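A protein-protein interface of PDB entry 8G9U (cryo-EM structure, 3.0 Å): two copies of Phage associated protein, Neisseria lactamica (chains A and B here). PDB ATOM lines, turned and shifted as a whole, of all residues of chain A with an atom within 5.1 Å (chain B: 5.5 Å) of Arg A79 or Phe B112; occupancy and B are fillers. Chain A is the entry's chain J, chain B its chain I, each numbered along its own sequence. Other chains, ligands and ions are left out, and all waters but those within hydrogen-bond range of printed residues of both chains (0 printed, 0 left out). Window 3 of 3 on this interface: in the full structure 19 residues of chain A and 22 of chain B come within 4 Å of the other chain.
The side-chain amide nitrogen (NE2) of Gln A75 is in hydrogen-bond range of the side-chain hydroxyl (OH) of Tyr B105, at 3.2 Å.
The backbone carbonyl oxygen (O) of Thr B108 is in hydrogen-bond range of the guanidinium group (NH1) of Arg A79.
The guanidinium group of Arg A79 lies close to the side-chain amide oxygen of Gln B109 (3.2 Å).
OE1 of Gln A80 lies within hydrogen-bond range of NE2 of Gln B109 (2.8 Å).
The side-chain amide nitrogen (NE2) of Gln B109 sits close to the side-chain carboxylate (OE2) of Glu A83 (3.0 Å).
The backbone carbonyl oxygen of Gln B109 sits close to the side-chain hydroxyl of Thr B113 (3.3 Å).
The indole nitrogen (NE1) of Trp A76 is in hydrogen-bond range of the side-chain amide oxygen (OE1) of Gln A80, at 3.4 Å.
The side-chain carboxylate (OE2) of Glu A83 sits close to the side-chain amide oxygen (OE1) of Gln A80 (2.7 Å).
Among the printed residues, merely in contact across the chains: Arg A79 with Phe B112 (3.0 Å), Arg A79 with Tyr B105 (3.3 Å), Leu A82 with Tyr B105 (3.4 Å) and Ile A78 with Tyr B105 (3.8 Å).
Of the printed residues of chain B, Gln A75 touches Tyr B105.
Arg A79 touches four residues of chain B.
Printed residues of chain A within 4 Å of Thr B108: Arg A79 (2.8 Å).
Printed residues of chain A within 4 Å of Gln B109: Arg A79 (3.0 Å), Gln A80 (2.8 Å) and Glu A83 (3.0 Å).
The nearest printed residue of chain A that does not touch Phe B112 is Trp A76 (6.3 Å).
Of the 10 printed residues of chain B, 4 touch a printed residue of chain A.
Printed residues of chain B that touch a printed residue of chain A: Tyr B105, Thr B108, Gln B109 and Phe B112.
Hydrophobic or aromatic side chains of chain B within 4 Å of the printed part of chain A: Tyr B105 and Phe B112.
Hydrophobic or aromatic side chains of chain A within 4 Å of the printed part of chain B: Ile A78 and Leu A82.
Among the printed residues, 9 pairs touch across the chains.
Among the printed residues, no Asp or Glu carboxylate lies within 4 Å of a Lys or Arg side-chain nitrogen of the other chain.
No position is printed for both chains.
Of the 9 pairs that touch across the chains among the printed residues, none has its exchanged pair printed and touching as well.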
ATOM      1  N   GLN A  75       4.574  18.330 -11.320  1.00  0.00           N
ATOM      2  CA  GLN A  75       4.177  19.261 -10.276  1.00  0.00           C
ATOM      3  C   GLN A  75       4.342  18.642  -8.901  1.00  0.00           C
ATOM      4  O   GLN A  75       4.695  19.338  -7.942  1.00  0.00           O
ATOM      5  CB  GLN A  75       2.735  19.700 -10.484  1.00  0.00           C
ATOM      6  CG  GLN A  75       2.384  20.945  -9.728  1.00  0.00           C
ATOM      7  CD  GLN A  75       1.054  21.512 -10.142  1.00  0.00           C
ATOM      8  OE1 GLN A  75       0.192  20.794 -10.644  1.00  0.00           O
ATOM      9  NE2 GLN A  75       0.878  22.811  -9.941  1.00  0.00           N
ATOM     10  N   TRP A  76       4.105  17.338  -8.783  1.00  0.00           N
ATOM     11  CA  TRP A  76       4.251  16.691  -7.493  1.00  0.00           C
ATOM     12  C   TRP A  76       5.685  16.770  -7.013  1.00  0.00           C
ATOM     13  O   TRP A  76       5.938  17.043  -5.840  1.00  0.00           O
ATOM     14  CB  TRP A  76       3.804  15.241  -7.569  1.00  0.00           C
ATOM     15  CG  TRP A  76       4.259  14.452  -6.404  1.00  0.00           C
ATOM     16  CD1 TRP A  76       3.653  14.366  -5.196  1.00  0.00           C
ATOM     17  CD2 TRP A  76       5.424  13.636  -6.326  1.00  0.00           C
ATOM     18  NE1 TRP A  76       4.362  13.545  -4.365  1.00  0.00           N
ATOM     19  CE2 TRP A  76       5.458  13.081  -5.039  1.00  0.00           C
ATOM     20  CE3 TRP A  76       6.440  13.316  -7.222  1.00  0.00           C
ATOM     21  CZ2 TRP A  76       6.464  12.229  -4.626  1.00  0.00           C
ATOM     22  CZ3 TRP A  76       7.439  12.474  -6.809  1.00  0.00           C
ATOM     23  CH2 TRP A  76       7.445  11.940  -5.524  1.00  0.00           C
ATOM     24  N   GLU A  77       6.644  16.537  -7.903  1.00  0.00           N
ATOM     25  CA  GLU A  77       8.022  16.631  -7.453  1.00  0.00           C
ATOM     26  C   GLU A  77       8.475  18.068  -7.311  1.00  0.00           C
ATOM     27  O   GLU A  77       9.408  18.326  -6.554  1.00  0.00           O
ATOM     28  CB  GLU A  77       8.956  15.893  -8.388  1.00  0.00           C
ATOM     29  CG  GLU A  77       8.801  16.312  -9.788  1.00  0.00           C
ATOM     30  CD  GLU A  77       9.972  15.905 -10.610  1.00  0.00           C
ATOM     31  OE1 GLU A  77      10.946  15.398 -10.022  1.00  0.00           O
ATOM     32  OE2 GLU A  77       9.915  16.089 -11.840  1.00  0.00           O
ATOM     33  N   ILE A  78       7.832  19.016  -7.988  1.00  0.00           N
ATOM     34  CA  ILE A  78       8.079  20.414  -7.650  1.00  0.00           C
ATOM     35  C   ILE A  78       7.689  20.670  -6.207  1.00  0.00           C
ATOM     36  O   ILE A  78       8.400  21.349  -5.464  1.00  0.00           O
ATOM     37  CB  ILE A  78       7.321  21.358  -8.588  1.00  0.00           C
ATOM     38  CG1 ILE A  78       7.832  21.232  -9.998  1.00  0.00           C
ATOM     39  CG2 ILE A  78       7.490  22.783  -8.139  1.00  0.00           C
ATOM     40  CD1 ILE A  78       6.940  21.903 -10.916  1.00  0.00           C
ATOM     41  N   ARG A  79       6.540  20.145  -5.795  1.00  0.00           N
ATOM     42  CA  ARG A  79       6.138  20.304  -4.403  1.00  0.00           C
ATOM     43  C   ARG A  79       7.075  19.549  -3.474  1.00  0.00           C
ATOM     44  O   ARG A  79       7.404  20.031  -2.385  1.00  0.00           O
ATOM     45  CB  ARG A  79       4.704  19.839  -4.217  1.00  0.00           C
ATOM     46  CG  ARG A  79       3.778  20.476  -5.194  1.00  0.00           C
ATOM     47  CD  ARG A  79       2.406  19.915  -5.083  1.00  0.00           C
ATOM     48  NE  ARG A  79       2.404  18.471  -5.207  1.00  0.00           N
ATOM     49  CZ  ARG A  79       1.569  17.695  -4.539  1.00  0.00           C
ATOM     50  NH1 ARG A  79       0.700  18.246  -3.716  1.00  0.00           N
ATOM     51  NH2 ARG A  79       1.601  16.384  -4.684  1.00  0.00           N
ATOM     52  N   GLN A  80       7.509  18.361  -3.886  1.00  0.00           N
ATOM     53  CA  GLN A  80       8.448  17.597  -3.077  1.00  0.00           C
ATOM     54  C   GLN A  80       9.731  18.376  -2.873  1.00  0.00           C
ATOM     55  O   GLN A  80      10.328  18.341  -1.794  1.00  0.00           O
ATOM     56  CB  GLN A  80       8.760  16.261  -3.734  1.00  0.00           C
ATOM     57  CG  GLN A  80       7.580  15.359  -3.888  1.00  0.00           C
ATOM     58  CD  GLN A  80       6.836  15.156  -2.598  1.00  0.00           C
ATOM     59  OE1 GLN A  80       5.857  15.845  -2.325  1.00  0.00           O
ATOM     60  NE2 GLN A  80       7.305  14.224  -1.782  1.00  0.00           N
ATOM     61  N   ILE A  81      10.185  19.060  -3.916  1.00  0.00           N
ATOM     62  CA  ILE A  81      11.357  19.912  -3.804  1.00  0.00           C
ATOM     63  C   ILE A  81      11.070  21.097  -2.902  1.00  0.00           C
ATOM     64  O   ILE A  81      11.851  21.414  -2.000  1.00  0.00           O
ATOM     65  CB  ILE A  81      11.798  20.370  -5.199  1.00  0.00           C
ATOM     66  CG1 ILE A  81      12.377  19.200  -5.977  1.00  0.00           C
ATOM     67  CG2 ILE A  81      12.789  21.460  -5.067  1.00  0.00           C
ATOM     68  CD1 ILE A  81      12.322  19.382  -7.452  1.00  0.00           C
ATOM     69  N   LEU A  82       9.945  21.759  -3.118  1.00  0.00           N
ATOM     70  CA  LEU A  82       9.659  23.005  -2.437  1.00  0.00           C
ATOM     71  C   LEU A  82       9.302  22.828  -0.974  1.00  0.00           C
ATOM     72  O   LEU A  82       9.330  23.811  -0.233  1.00  0.00           O
ATOM     73  CB  LEU A  82       8.546  23.757  -3.161  1.00  0.00           C
ATOM     74  CG  LEU A  82       9.099  24.379  -4.436  1.00  0.00           C
ATOM     75  CD1 LEU A  82       8.057  25.160  -5.173  1.00  0.00           C
ATOM     76  CD2 LEU A  82      10.247  25.274  -4.070  1.00  0.00           C
ATOM     77  N   GLU A  83       8.986  21.613  -0.525  1.00  0.00           N
ATOM     78  CA  GLU A  83       8.935  21.398   0.915  1.00  0.00           C
ATOM     79  C   GLU A  83      10.274  21.738   1.545  1.00  0.00           C
ATOM     80  O   GLU A  83      10.336  22.200   2.689  1.00  0.00           O
ATOM     81  CB  GLU A  83       8.567  19.961   1.256  1.00  0.00           C
ATOM     82  CG  GLU A  83       7.212  19.514   0.808  1.00  0.00           C
ATOM     83  CD  GLU A  83       7.246  18.082   0.344  1.00  0.00           C
ATOM     84  OE1 GLU A  83       8.128  17.330   0.812  1.00  0.00           O
ATOM     85  OE2 GLU A  83       6.407  17.704  -0.491  1.00  0.00           O
ATOM     86  N   LYS B  22      -6.907  24.444  -5.389  1.00  0.00           N
ATOM     87  CA  LYS B  22      -7.369  23.134  -4.963  1.00  0.00           C
ATOM     88  C   LYS B  22      -8.878  23.063  -5.023  1.00  0.00           C
ATOM     89  O   LYS B  22      -9.449  22.069  -5.481  1.00  0.00           O
ATOM     90  CB  LYS B  22      -6.878  22.829  -3.558  1.00  0.00           C
ATOM     91  CG  LYS B  22      -7.131  21.410  -3.160  1.00  0.00           C
ATOM     92  CD  LYS B  22      -6.237  20.482  -3.924  1.00  0.00           C
ATOM     93  CE  LYS B  22      -6.818  19.095  -3.946  1.00  0.00           C
ATOM     94  NZ  LYS B  22      -7.028  18.580  -2.572  1.00  0.00           N
ATOM     95  N   TYR B 105       3.208  25.787  -3.628  1.00  0.00           N
ATOM     96  CA  TYR B 105       3.551  24.378  -3.676  1.00  0.00           C
ATOM     97  C   TYR B 105       3.616  23.724  -2.305  1.00  0.00           C
ATOM     98  O   TYR B 105       3.289  22.543  -2.189  1.00  0.00           O
ATOM     99  CB  TYR B 105       4.837  24.206  -4.460  1.00  0.00           C
ATOM    100  CG  TYR B 105       4.518  24.324  -5.919  1.00  0.00           C
ATOM    101  CD1 TYR B 105       3.610  23.472  -6.496  1.00  0.00           C
ATOM    102  CD2 TYR B 105       5.024  25.343  -6.685  1.00  0.00           C
ATOM    103  CE1 TYR B 105       3.278  23.570  -7.799  1.00  0.00           C
ATOM    104  CE2 TYR B 105       4.687  25.461  -8.004  1.00  0.00           C
ATOM    105  CZ  TYR B 105       3.808  24.566  -8.556  1.00  0.00           C
ATOM    106  OH  TYR B 105       3.439  24.653  -9.873  1.00  0.00           O
ATOM    107  N   GLU B 107       1.472  24.546   0.244  1.00  0.00           N
ATOM    108  CA  GLU B 107       0.081  24.287   0.571  1.00  0.00           C
ATOM    109  C   GLU B 107      -0.530  23.290  -0.392  1.00  0.00           C
ATOM    110  O   GLU B 107      -1.418  22.527  -0.015  1.00  0.00           O
ATOM    111  CB  GLU B 107      -0.708  25.585   0.561  1.00  0.00           C
ATOM    112  CG  GLU B 107      -2.138  25.440   0.997  1.00  0.00           C
ATOM    113  CD  GLU B 107      -2.295  25.564   2.492  1.00  0.00           C
ATOM    114  OE1 GLU B 107      -1.475  26.257   3.124  1.00  0.00           O
ATOM    115  OE2 GLU B 107      -3.236  24.967   3.042  1.00  0.00           O
ATOM    116  N   THR B 108      -0.067  23.266  -1.638  1.00  0.00           N
ATOM    117  CA  THR B 108      -0.553  22.252  -2.555  1.00  0.00           C
ATOM    118  C   THR B 108      -0.135  20.874  -2.081  1.00  0.00           C
ATOM    119  O   THR B 108      -0.923  19.927  -2.133  1.00  0.00           O
ATOM    120  CB  THR B 108      -0.033  22.527  -3.958  1.00  0.00           C
ATOM    121  OG1 THR B 108      -0.403  23.851  -4.338  1.00  0.00           O
ATOM    122  CG2 THR B 108      -0.671  21.592  -4.927  1.00  0.00           C
ATOM    123  N   GLN B 109       1.095  20.746  -1.586  1.00  0.00           N
ATOM    124  CA  GLN B 109       1.495  19.492  -0.967  1.00  0.00           C
ATOM    125  C   GLN B 109       0.617  19.179   0.230  1.00  0.00           C
ATOM    126  O   GLN B 109       0.099  18.068   0.360  1.00  0.00           O
ATOM    127  CB  GLN B 109       2.958  19.553  -0.550  1.00  0.00           C
ATOM    128  CG  GLN B 109       3.438  18.286   0.098  1.00  0.00           C
ATOM    129  CD  GLN B 109       3.521  17.127  -0.864  1.00  0.00           C
ATOM    130  OE1 GLN B 109       3.236  17.263  -2.051  1.00  0.00           O
ATOM    131  NE2 GLN B 109       3.931  15.974  -0.356  1.00  0.00           N
ATOM    132  N   PHE B 110       0.411  20.166   1.094  1.00  0.00           N
ATOM    133  CA  PHE B 110      -0.396  19.950   2.284  1.00  0.00           C
ATOM    134  C   PHE B 110      -1.800  19.493   1.930  1.00  0.00           C
ATOM    135  O   PHE B 110      -2.411  18.724   2.676  1.00  0.00           O
ATOM    136  CB  PHE B 110      -0.443  21.227   3.108  1.00  0.00           C
ATOM    137  CG  PHE B 110      -1.536  21.252   4.114  1.00  0.00           C
ATOM    138  CD1 PHE B 110      -1.420  20.554   5.293  1.00  0.00           C
ATOM    139  CD2 PHE B 110      -2.679  21.985   3.887  1.00  0.00           C
ATOM    140  CE1 PHE B 110      -2.425  20.582   6.217  1.00  0.00           C
ATOM    141  CE2 PHE B 110      -3.684  22.014   4.809  1.00  0.00           C
ATOM    142  CZ  PHE B 110      -3.559  21.312   5.973  1.00  0.00           C
ATOM    143  N   LEU B 111      -2.326  19.956   0.803  1.00  0.00           N
ATOM    144  CA  LEU B 111      -3.653  19.541   0.374  1.00  0.00           C
ATOM    145  C   LEU B 111      -3.634  18.167  -0.267  1.00  0.00           C
ATOM    146  O   LEU B 111      -4.595  17.406  -0.125  1.00  0.00           O
ATOM    147  CB  LEU B 111      -4.231  20.571  -0.585  1.00  0.00           C
ATOM    148  CG  LEU B 111      -4.368  21.854   0.208  1.00  0.00           C
ATOM    149  CD1 LEU B 111      -4.973  22.957  -0.598  1.00  0.00           C
ATOM    150  CD2 LEU B 111      -5.188  21.536   1.415  1.00  0.00           C
ATOM    151  N   PHE B 112      -2.568  17.833  -0.979  1.00  0.00           N
ATOM    152  CA  PHE B 112      -2.471  16.536  -1.619  1.00  0.00           C
ATOM    153  C   PHE B 112      -1.758  15.499  -0.767  1.00  0.00           C
ATOM    154  O   PHE B 112      -1.630  14.354  -1.201  1.00  0.00           O
ATOM    155  CB  PHE B 112      -1.778  16.661  -2.970  1.00  0.00           C
ATOM    156  CG  PHE B 112      -2.604  17.345  -4.014  1.00  0.00           C
ATOM    157  CD1 PHE B 112      -3.496  16.635  -4.777  1.00  0.00           C
ATOM    158  CD2 PHE B 112      -2.475  18.692  -4.245  1.00  0.00           C
ATOM    159  CE1 PHE B 112      -4.245  17.261  -5.740  1.00  0.00           C
ATOM    160  CE2 PHE B 112      -3.222  19.316  -5.206  1.00  0.00           C
ATOM    161  CZ  PHE B 112      -4.103  18.601  -5.954  1.00  0.00           C
ATOM    162  N   THR B 113      -1.270  15.862   0.414  1.00  0.00           N
ATOM    163  CA  THR B 113      -1.002  14.844   1.418  1.00  0.00           C
ATOM    164  C   THR B 113      -2.328  14.365   1.980  1.00  0.00           C
ATOM    165  O   THR B 113      -3.202  15.172   2.299  1.00  0.00           O
ATOM    166  CB  THR B 113      -0.097  15.374   2.525  1.00  0.00           C
ATOM    167  OG1 THR B 113      -0.735  16.473   3.176  1.00  0.00           O
ATOM    168  CG2 THR B 113       1.262  15.785   1.987  1.00  0.00           C
ATOM    169  N   LYS B 114      -2.466  13.047   2.110  1.00  0.00           N
ATOM    170  CA  LYS B 114      -3.769  12.397   2.146  1.00  0.00           C
ATOM    171  C   LYS B 114      -4.702  12.965   3.202  1.00  0.00           C
ATOM    172  O   LYS B 114      -5.733  13.555   2.871  1.00  0.00           O
ATOM    173  CB  LYS B 114      -3.592  10.895   2.368  1.00  0.00           C
ATOM    174  CG  LYS B 114      -4.881  10.099   2.296  1.00  0.00           C
ATOM    175  CD  LYS B 114      -4.627   8.616   2.501  1.00  0.00           C
ATOM    176  CE  LYS B 114      -3.565   8.113   1.534  1.00  0.00           C
ATOM    177  NZ  LYS B 114      -3.264   6.666   1.705  1.00  0.00           N
